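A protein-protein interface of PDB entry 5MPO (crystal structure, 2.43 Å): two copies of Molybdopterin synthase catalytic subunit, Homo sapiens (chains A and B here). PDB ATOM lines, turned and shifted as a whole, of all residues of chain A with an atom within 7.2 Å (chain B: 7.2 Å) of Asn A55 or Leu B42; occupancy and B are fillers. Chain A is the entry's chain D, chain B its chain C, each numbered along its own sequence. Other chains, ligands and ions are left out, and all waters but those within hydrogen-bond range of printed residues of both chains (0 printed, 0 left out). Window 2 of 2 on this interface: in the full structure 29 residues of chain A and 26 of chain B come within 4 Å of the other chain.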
ATOM      1  N   THR A  52      21.378  -2.156 -17.960  1.00  0.00           N
ATOM      2  CA  THR A  52      20.716  -3.441 -17.838  1.00  0.00           C
ATOM      3  C   THR A  52      21.765  -4.459 -17.479  1.00  0.00           C
ATOM      4  O   THR A  52      22.938  -4.307 -17.817  1.00  0.00           O
ATOM      5  CB  THR A  52      20.086  -3.926 -19.199  1.00  0.00           C
ATOM      6  OG1 THR A  52      21.079  -3.909 -20.244  1.00  0.00           O
ATOM      7  CG2 THR A  52      18.948  -3.067 -19.596  1.00  0.00           C
ATOM      8  N   THR A  53      21.336  -5.535 -16.862  1.00  0.00           N
ATOM      9  CA  THR A  53      22.273  -6.591 -16.454  1.00  0.00           C
ATOM     10  C   THR A  53      22.658  -7.425 -17.680  1.00  0.00           C
ATOM     11  O   THR A  53      21.793  -7.978 -18.396  1.00  0.00           O
ATOM     12  CB  THR A  53      21.636  -7.434 -15.325  1.00  0.00           C
ATOM     13  OG1 THR A  53      21.368  -6.568 -14.225  1.00  0.00           O
ATOM     14  CG2 THR A  53      22.507  -8.546 -14.874  1.00  0.00           C
ATOM     15  N   ARG A  54      23.957  -7.433 -17.945  1.00  0.00           N
ATOM     16  CA  ARG A  54      24.604  -8.305 -18.909  1.00  0.00           C
ATOM     17  C   ARG A  54      24.699  -9.675 -18.342  1.00  0.00           C
ATOM     18  O   ARG A  54      24.683  -9.826 -17.140  1.00  0.00           O
ATOM     19  CB  ARG A  54      26.054  -7.896 -19.158  1.00  0.00           C
ATOM     20  CG  ARG A  54      26.199  -6.609 -19.871  1.00  0.00           C
ATOM     21  CD  ARG A  54      27.426  -6.612 -20.742  1.00  0.00           C
ATOM     22  NE  ARG A  54      28.602  -6.398 -19.931  1.00  0.00           N
ATOM     23  CZ  ARG A  54      29.699  -7.150 -19.925  1.00  0.00           C
ATOM     24  NH1 ARG A  54      29.840  -8.204 -20.726  1.00  0.00           N
ATOM     25  NH2 ARG A  54      30.692  -6.828 -19.107  1.00  0.00           N
ATOM     26  N   ASN A  55      24.874 -10.646 -19.229  1.00  0.00           N
ATOM     27  CA  ASN A  55      24.889 -12.045 -18.867  1.00  0.00           C
ATOM     28  C   ASN A  55      26.315 -12.598 -18.752  1.00  0.00           C
ATOM     29  O   ASN A  55      26.518 -13.801 -18.764  1.00  0.00           O
ATOM     30  CB  ASN A  55      24.077 -12.842 -19.887  1.00  0.00           C
ATOM     31  CG  ASN A  55      24.783 -13.009 -21.212  1.00  0.00           C
ATOM     32  OD1 ASN A  55      25.867 -12.510 -21.431  1.00  0.00           O
ATOM     33  ND2 ASN A  55      24.164 -13.727 -22.101  1.00  0.00           N
ATOM     34  N   ASN A  56      27.312 -11.735 -18.675  1.00  0.00           N
ATOM     35  CA  ASN A  56      28.670 -12.226 -18.652  1.00  0.00           C
ATOM     36  C   ASN A  56      29.575 -11.166 -18.086  1.00  0.00           C
ATOM     37  O   ASN A  56      29.331  -9.977 -18.246  1.00  0.00           O
ATOM     38  CB  ASN A  56      29.144 -12.653 -20.035  1.00  0.00           C
ATOM     39  CG  ASN A  56      29.317 -11.477 -20.977  1.00  0.00           C
ATOM     40  OD1 ASN A  56      30.339 -10.776 -20.967  1.00  0.00           O
ATOM     41  ND2 ASN A  56      28.317 -11.251 -21.791  1.00  0.00           N
ATOM     42  N   PHE A  57      30.578 -11.607 -17.353  1.00  0.00           N
ATOM     43  CA  PHE A  57      31.530 -10.699 -16.772  1.00  0.00           C
ATOM     44  C   PHE A  57      32.881 -11.404 -16.679  1.00  0.00           C
ATOM     45  O   PHE A  57      32.968 -12.538 -16.173  1.00  0.00           O
ATOM     46  CB  PHE A  57      31.021 -10.218 -15.417  1.00  0.00           C
ATOM     47  CG  PHE A  57      31.886  -9.157 -14.799  1.00  0.00           C
ATOM     48  CD1 PHE A  57      31.850  -7.855 -15.273  1.00  0.00           C
ATOM     49  CD2 PHE A  57      32.759  -9.469 -13.743  1.00  0.00           C
ATOM     50  CE1 PHE A  57      32.667  -6.876 -14.710  1.00  0.00           C
ATOM     51  CE2 PHE A  57      33.569  -8.501 -13.173  1.00  0.00           C
ATOM     52  CZ  PHE A  57      33.524  -7.200 -13.654  1.00  0.00           C
ATOM     53  N   GLY A  59      34.422 -13.060 -18.731  1.00  0.00           N
ATOM     54  CA  GLY A  59      34.341 -14.424 -19.246  1.00  0.00           C
ATOM     55  C   GLY A  59      33.483 -15.420 -18.476  1.00  0.00           C
ATOM     56  O   GLY A  59      33.270 -16.506 -18.957  1.00  0.00           O
ATOM     57  N   LYS A  60      32.960 -15.075 -17.313  1.00  0.00           N
ATOM     58  CA  LYS A  60      32.088 -15.989 -16.580  1.00  0.00           C
ATOM     59  C   LYS A  60      30.634 -15.637 -16.954  1.00  0.00           C
ATOM     60  O   LYS A  60      30.376 -14.500 -17.347  1.00  0.00           O
ATOM     61  CB  LYS A  60      32.332 -15.848 -15.078  1.00  0.00           C
ATOM     62  CG  LYS A  60      33.815 -15.738 -14.659  1.00  0.00           C
ATOM     63  CD  LYS A  60      33.989 -15.477 -13.154  1.00  0.00           C
ATOM     64  CE  LYS A  60      34.832 -14.232 -12.837  1.00  0.00           C
ATOM     65  NZ  LYS A  60      36.307 -14.486 -12.853  1.00  0.00           N
ATOM     66  N   LYS A  61      29.697 -16.596 -16.859  1.00  0.00           N
ATOM     67  CA  LYS A  61      28.295 -16.315 -17.122  1.00  0.00           C
ATOM     68  C   LYS A  61      27.671 -15.776 -15.873  1.00  0.00           C
ATOM     69  O   LYS A  61      27.972 -16.267 -14.788  1.00  0.00           O
ATOM     70  CB  LYS A  61      27.529 -17.535 -17.633  1.00  0.00           C
ATOM     71  N   VAL A  62      26.781 -14.783 -16.044  1.00  0.00           N
ATOM     72  CA  VAL A  62      26.126 -13.994 -14.959  1.00  0.00           C
ATOM     73  C   VAL A  62      24.584 -14.186 -15.037  1.00  0.00           C
ATOM     74  O   VAL A  62      24.001 -14.036 -16.120  1.00  0.00           O
ATOM     75  CB  VAL A  62      26.484 -12.454 -15.049  1.00  0.00           C
ATOM     76  CG1 VAL A  62      25.699 -11.605 -14.065  1.00  0.00           C
ATOM     77  CG2 VAL A  62      27.967 -12.200 -14.834  1.00  0.00           C
ATOM     78  N   ILE A  63      23.962 -14.506 -13.889  1.00  0.00           N
ATOM     79  CA  ILE A  63      22.515 -14.709 -13.727  1.00  0.00           C
ATOM     80  C   ILE A  63      21.861 -13.431 -13.197  1.00  0.00           C
ATOM     81  O   ILE A  63      20.683 -13.163 -13.431  1.00  0.00           O
ATOM     82  CB  ILE A  63      22.208 -15.871 -12.721  1.00  0.00           C
ATOM     83  N   SER A  64      22.597 -12.636 -12.444  1.00  0.00           N
ATOM     84  CA  SER A  64      21.990 -11.467 -11.845  1.00  0.00           C
ATOM     85  C   SER A  64      23.044 -10.461 -11.379  1.00  0.00           C
ATOM     86  O   SER A  64      24.254 -10.762 -11.373  1.00  0.00           O
ATOM     87  CB  SER A  64      21.131 -11.899 -10.661  1.00  0.00           C
ATOM     88  OG  SER A  64      20.256 -10.862 -10.266  1.00  0.00           O
ATOM     89  N   VAL A 105      19.255 -10.653 -15.564  1.00  0.00           N
ATOM     90  CA  VAL A 105      19.729 -10.450 -16.901  1.00  0.00           C
ATOM     91  C   VAL A 105      18.635  -9.771 -17.704  1.00  0.00           C
ATOM     92  O   VAL A 105      17.464 -10.145 -17.627  1.00  0.00           O
ATOM     93  CB  VAL A 105      20.185 -11.776 -17.562  1.00  0.00           C
ATOM     94  CG1 VAL A 105      20.380 -11.619 -19.064  1.00  0.00           C
ATOM     95  CG2 VAL A 105      21.491 -12.251 -16.935  1.00  0.00           C
ATOM     96  N   SER A 106      19.050  -8.730 -18.425  1.00  0.00           N
ATOM     97  CA  SER A 106      18.197  -7.968 -19.358  1.00  0.00           C
ATOM     98  C   SER A 106      17.162  -7.127 -18.684  1.00  0.00           C
ATOM     99  O   SER A 106      16.278  -6.672 -19.350  1.00  0.00           O
ATOM    100  CB  SER A 106      17.526  -8.883 -20.395  1.00  0.00           C
ATOM    101  OG  SER A 106      18.469  -9.146 -21.416  1.00  0.00           O
ATOM    102  N   GLU B  15      24.591 -17.363 -30.187  1.00  0.00           N
ATOM    103  CA  GLU B  15      24.714 -16.467 -31.366  1.00  0.00           C
ATOM    104  C   GLU B  15      23.404 -15.699 -31.651  1.00  0.00           C
ATOM    105  O   GLU B  15      22.523 -16.218 -32.346  1.00  0.00           O
ATOM    106  CB  GLU B  15      25.140 -17.291 -32.594  1.00  0.00           C
ATOM    107  CG  GLU B  15      25.320 -16.480 -33.865  1.00  0.00           C
ATOM    108  CD  GLU B  15      26.181 -15.253 -33.648  1.00  0.00           C
ATOM    109  OE1 GLU B  15      27.323 -15.420 -33.148  1.00  0.00           O
ATOM    110  OE2 GLU B  15      25.709 -14.134 -33.965  1.00  0.00           O
ATOM    111  N   GLU B  16      23.283 -14.482 -31.102  1.00  0.00           N
ATOM    112  CA  GLU B  16      22.155 -13.529 -31.385  1.00  0.00           C
ATOM    113  C   GLU B  16      22.517 -12.611 -32.555  1.00  0.00           C
ATOM    114  O   GLU B  16      23.525 -11.911 -32.491  1.00  0.00           O
ATOM    115  CB  GLU B  16      21.906 -12.678 -30.148  1.00  0.00           C
ATOM    116  CG  GLU B  16      20.730 -11.725 -30.176  1.00  0.00           C
ATOM    117  CD  GLU B  16      20.733 -10.790 -28.974  1.00  0.00           C
ATOM    118  OE1 GLU B  16      21.757 -10.689 -28.280  1.00  0.00           O
ATOM    119  OE2 GLU B  16      19.711 -10.129 -28.707  1.00  0.00           O
ATOM    120  N   ILE B  39      16.875  -4.590 -26.598  1.00  0.00           N
ATOM    121  CA  ILE B  39      17.424  -5.301 -25.443  1.00  0.00           C
ATOM    122  C   ILE B  39      18.244  -6.526 -25.871  1.00  0.00           C
ATOM    123  O   ILE B  39      17.896  -7.198 -26.812  1.00  0.00           O
ATOM    124  CB  ILE B  39      16.284  -5.779 -24.526  1.00  0.00           C
ATOM    125  CG1 ILE B  39      15.735  -4.592 -23.744  1.00  0.00           C
ATOM    126  CG2 ILE B  39      16.765  -6.853 -23.538  1.00  0.00           C
ATOM    127  CD1 ILE B  39      14.363  -4.828 -23.143  1.00  0.00           C
ATOM    128  N   SER B  40      19.324  -6.801 -25.156  1.00  0.00           N
ATOM    129  CA  SER B  40      20.212  -7.921 -25.459  1.00  0.00           C
ATOM    130  C   SER B  40      20.886  -8.368 -24.183  1.00  0.00           C
ATOM    131  O   SER B  40      21.511  -7.550 -23.506  1.00  0.00           O
ATOM    132  CB  SER B  40      21.293  -7.538 -26.500  1.00  0.00           C
ATOM    133  OG  SER B  40      22.264  -8.582 -26.725  1.00  0.00           O
ATOM    134  N   PRO B  41      20.826  -9.673 -23.871  1.00  0.00           N
ATOM    135  CA  PRO B  41      21.560 -10.174 -22.690  1.00  0.00           C
ATOM    136  C   PRO B  41      23.059  -9.913 -22.776  1.00  0.00           C
ATOM    137  O   PRO B  41      23.729  -9.900 -21.774  1.00  0.00           O
ATOM    138  CB  PRO B  41      21.255 -11.677 -22.687  1.00  0.00           C
ATOM    139  CG  PRO B  41      20.900 -12.013 -24.110  1.00  0.00           C
ATOM    140  CD  PRO B  41      20.315 -10.772 -24.716  1.00  0.00           C
ATOM    141  N   LEU B  42      23.582  -9.685 -23.963  1.00  0.00           N
ATOM    142  CA  LEU B  42      24.979  -9.279 -24.092  1.00  0.00           C
ATOM    143  C   LEU B  42      25.192  -7.783 -23.872  1.00  0.00           C
ATOM    144  O   LEU B  42      26.319  -7.350 -23.922  1.00  0.00           O
ATOM    145  CB  LEU B  42      25.507  -9.633 -25.471  1.00  0.00           C
ATOM    146  CG  LEU B  42      25.420 -11.132 -25.808  1.00  0.00           C
ATOM    147  CD1 LEU B  42      25.357 -11.328 -27.322  1.00  0.00           C
ATOM    148  CD2 LEU B  42      26.570 -11.928 -25.183  1.00  0.00           C
ATOM    149  N   CYS B  43      24.124  -7.010 -23.638  1.00  0.00           N
ATOM    150  CA  CYS B  43      24.193  -5.563 -23.586  1.00  0.00           C
ATOM    151  C   CYS B  43      23.832  -5.045 -22.224  1.00  0.00           C
ATOM    152  O   CYS B  43      22.830  -5.471 -21.632  1.00  0.00           O
ATOM    153  CB  CYS B  43      23.268  -4.940 -24.642  1.00  0.00           C
ATOM    154  SG  CYS B  43      24.031  -5.122 -26.268  1.00  0.00           S
ATOM    155  N   GLY B  44      24.679  -4.132 -21.750  1.00  0.00           N
ATOM    156  CA  GLY B  44      24.515  -3.406 -20.506  1.00  0.00           C
ATOM    157  C   GLY B  44      23.956  -2.004 -20.644  1.00  0.00           C
ATOM    158  O   GLY B  44      23.519  -1.427 -19.652  1.00  0.00           O
ATOM    159  N   ALA B  45      23.952  -1.448 -21.854  1.00  0.00           N
ATOM    160  CA  ALA B  45      23.540  -0.038 -22.047  1.00  0.00           C
ATOM    161  C   ALA B  45      22.599   0.144 -23.256  1.00  0.00           C
ATOM    162  O   ALA B  45      22.854  -0.378 -24.330  1.00  0.00           O
ATOM    163  CB  ALA B  45      24.766   0.850 -22.204  1.00  0.00           C
ATOM    164  N   LYS B  92      25.139  -3.392 -30.593  1.00  0.00           N
ATOM    165  CA  LYS B  92      24.478  -4.620 -30.932  1.00  0.00           C
ATOM    166  C   LYS B  92      23.306  -4.369 -31.885  1.00  0.00           C
ATOM    167  O   LYS B  92      23.431  -4.673 -33.057  1.00  0.00           O
ATOM    168  CB  LYS B  92      24.024  -5.341 -29.669  1.00  0.00           C
ATOM    169  CG  LYS B  92      23.464  -6.725 -29.928  1.00  0.00           C
ATOM    170  CD  LYS B  92      24.472  -7.566 -30.705  1.00  0.00           C
ATOM    171  CE  LYS B  92      24.096  -9.033 -30.741  1.00  0.00           C
ATOM    172  NZ  LYS B  92      24.992  -9.745 -31.689  1.00  0.00           N
ATOM    173  N   SER B 116      24.470  -1.608 -26.521  1.00  0.00           N
ATOM    174  CA  SER B 116      25.852  -2.116 -26.644  1.00  0.00           C
ATOM    175  C   SER B 116      26.318  -2.648 -25.278  1.00  0.00           C
ATOM    176  O   SER B 116      25.652  -2.461 -24.274  1.00  0.00           O
ATOM    177  CB  SER B 116      26.803  -1.003 -27.091  1.00  0.00           C
ATOM    178  OG  SER B 116      26.711   0.080 -26.179  1.00  0.00           O
ATOM    179  N   ALA B 117      27.484  -3.267 -25.264  1.00  0.00           N
ATOM    180  CA  ALA B 117      28.070  -3.819 -24.035  1.00  0.00           C
ATOM    181  C   ALA B 117      28.394  -2.725 -23.010  1.00  0.00           C
ATOM    182  O   ALA B 117      28.014  -2.890 -21.807  1.00  0.00           O
ATOM    183  CB  ALA B 117      29.284  -4.728 -24.349  1.00  0.00           C
ATOM    184  N   HIS B 118      29.020  -1.627 -23.473  1.00  0.00           N
ATOM    185  CA  HIS B 118      29.321  -0.450 -22.629  1.00  0.00           C
ATOM    186  C   HIS B 118      28.746   0.912 -23.166  1.00  0.00           C
ATOM    187  O   HIS B 118      28.404   1.080 -24.331  1.00  0.00           O
ATOM    188  CB  HIS B 118      30.837  -0.357 -22.372  1.00  0.00           C
ATOM    189  CG  HIS B 118      31.442  -1.574 -21.698  1.00  0.00           C
ATOM    190  ND1 HIS B 118      31.033  -2.037 -20.462  1.00  0.00           N
ATOM    191  CD2 HIS B 118      32.463  -2.390 -22.073  1.00  0.00           C
ATOM    192  CE1 HIS B 118      31.759  -3.087 -20.114  1.00  0.00           C
ATOM    193  NE2 HIS B 118      32.629  -3.325 -21.077  1.00  0.00           N
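Along chain A the printed residues that touch a printed residue of chain B span positions 52 to 106. Of the 13 printed residues of chain B, 7 touch a printed residue of chain A. Along chain B the printed residues that touch a printed residue of chain A span positions 39 to 117. Among the printed residues, 14 pairs touch across the chains. Among the printed residues, no Asp or Glu carboxylate lies within 4 Å of a Lys or Arg side-chain nitrogen of the other chain.
Of the printed residues of chain B, Asn A55 touches Pro B41 (2.9 Å) and Leu B42 (3.9 Å). Glu B15 touches none of the printed residues of chain A. Of the printed residues of chain A, Ser B40 touches Ser A106. Leu B42 touches just these residues of chain A: Arg A54 (3.4 Å), Asn A55 (3.9 Å) and Asn A56 (3.9 Å). Of the printed residues of chain A, Gly B44 touches Thr A52 and Arg A54. Ala B45 touches none of the printed residues of chain A.
Among the printed residues, pairs that only touch across the chains: Arg A54 with Pro B41, Arg A54 with Leu B42, Arg A54 with Gly B44, Ser A106 with Ile B39, Arg A54 with Cys B43, Val A105 with Pro B41, Ser A106 with Ser B40, Asn A55 with Leu B42, Asn A56 with Leu B42 and Arg A54 with Ala B117.
OD1 of Asn A55 lies within hydrogen-bond range of ND2 of Asn A56, 2.8 Å away. NH1 of Arg A54 sits at hydrogen-bond distance from OD1 of Asn A56. N of Val A62 sits at hydrogen-bond distance from O of Asn A55 (2.9 Å). The backbone NH (N) of Ser B116 sits close to the side-chain sulfur (SG) of Cys B43 (3.6 Å). OG of Ser B40 sits close to N of Leu B42, at 3.3 Å. The side-chain carboxylate of Glu B16 lies within hydrogen-bond range of the side-chain hydroxyl of Ser B40.
No position is printed for both chains. Of the 14 pairs that touch across the chains among the printed residues, none has its exchanged pair printed and touching as well.
The backbone carbonyl oxygen of Pro B41 sits at hydrogen-bond distance from the backbone NH of Asn A55. The backbone nitrogen of Pro B41 sits close to the side-chain hydroxyl of Ser A106, at 3.4 Å. The backbone carbonyl oxygen of Gly B44 is in hydrogen-bond range of the backbone NH of Thr A52 (2.8 Å). The side-chain hydroxyl of Thr A52 is in hydrogen-bond range of the backbone carbonyl oxygen of Cys B43 (2.7 Å).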
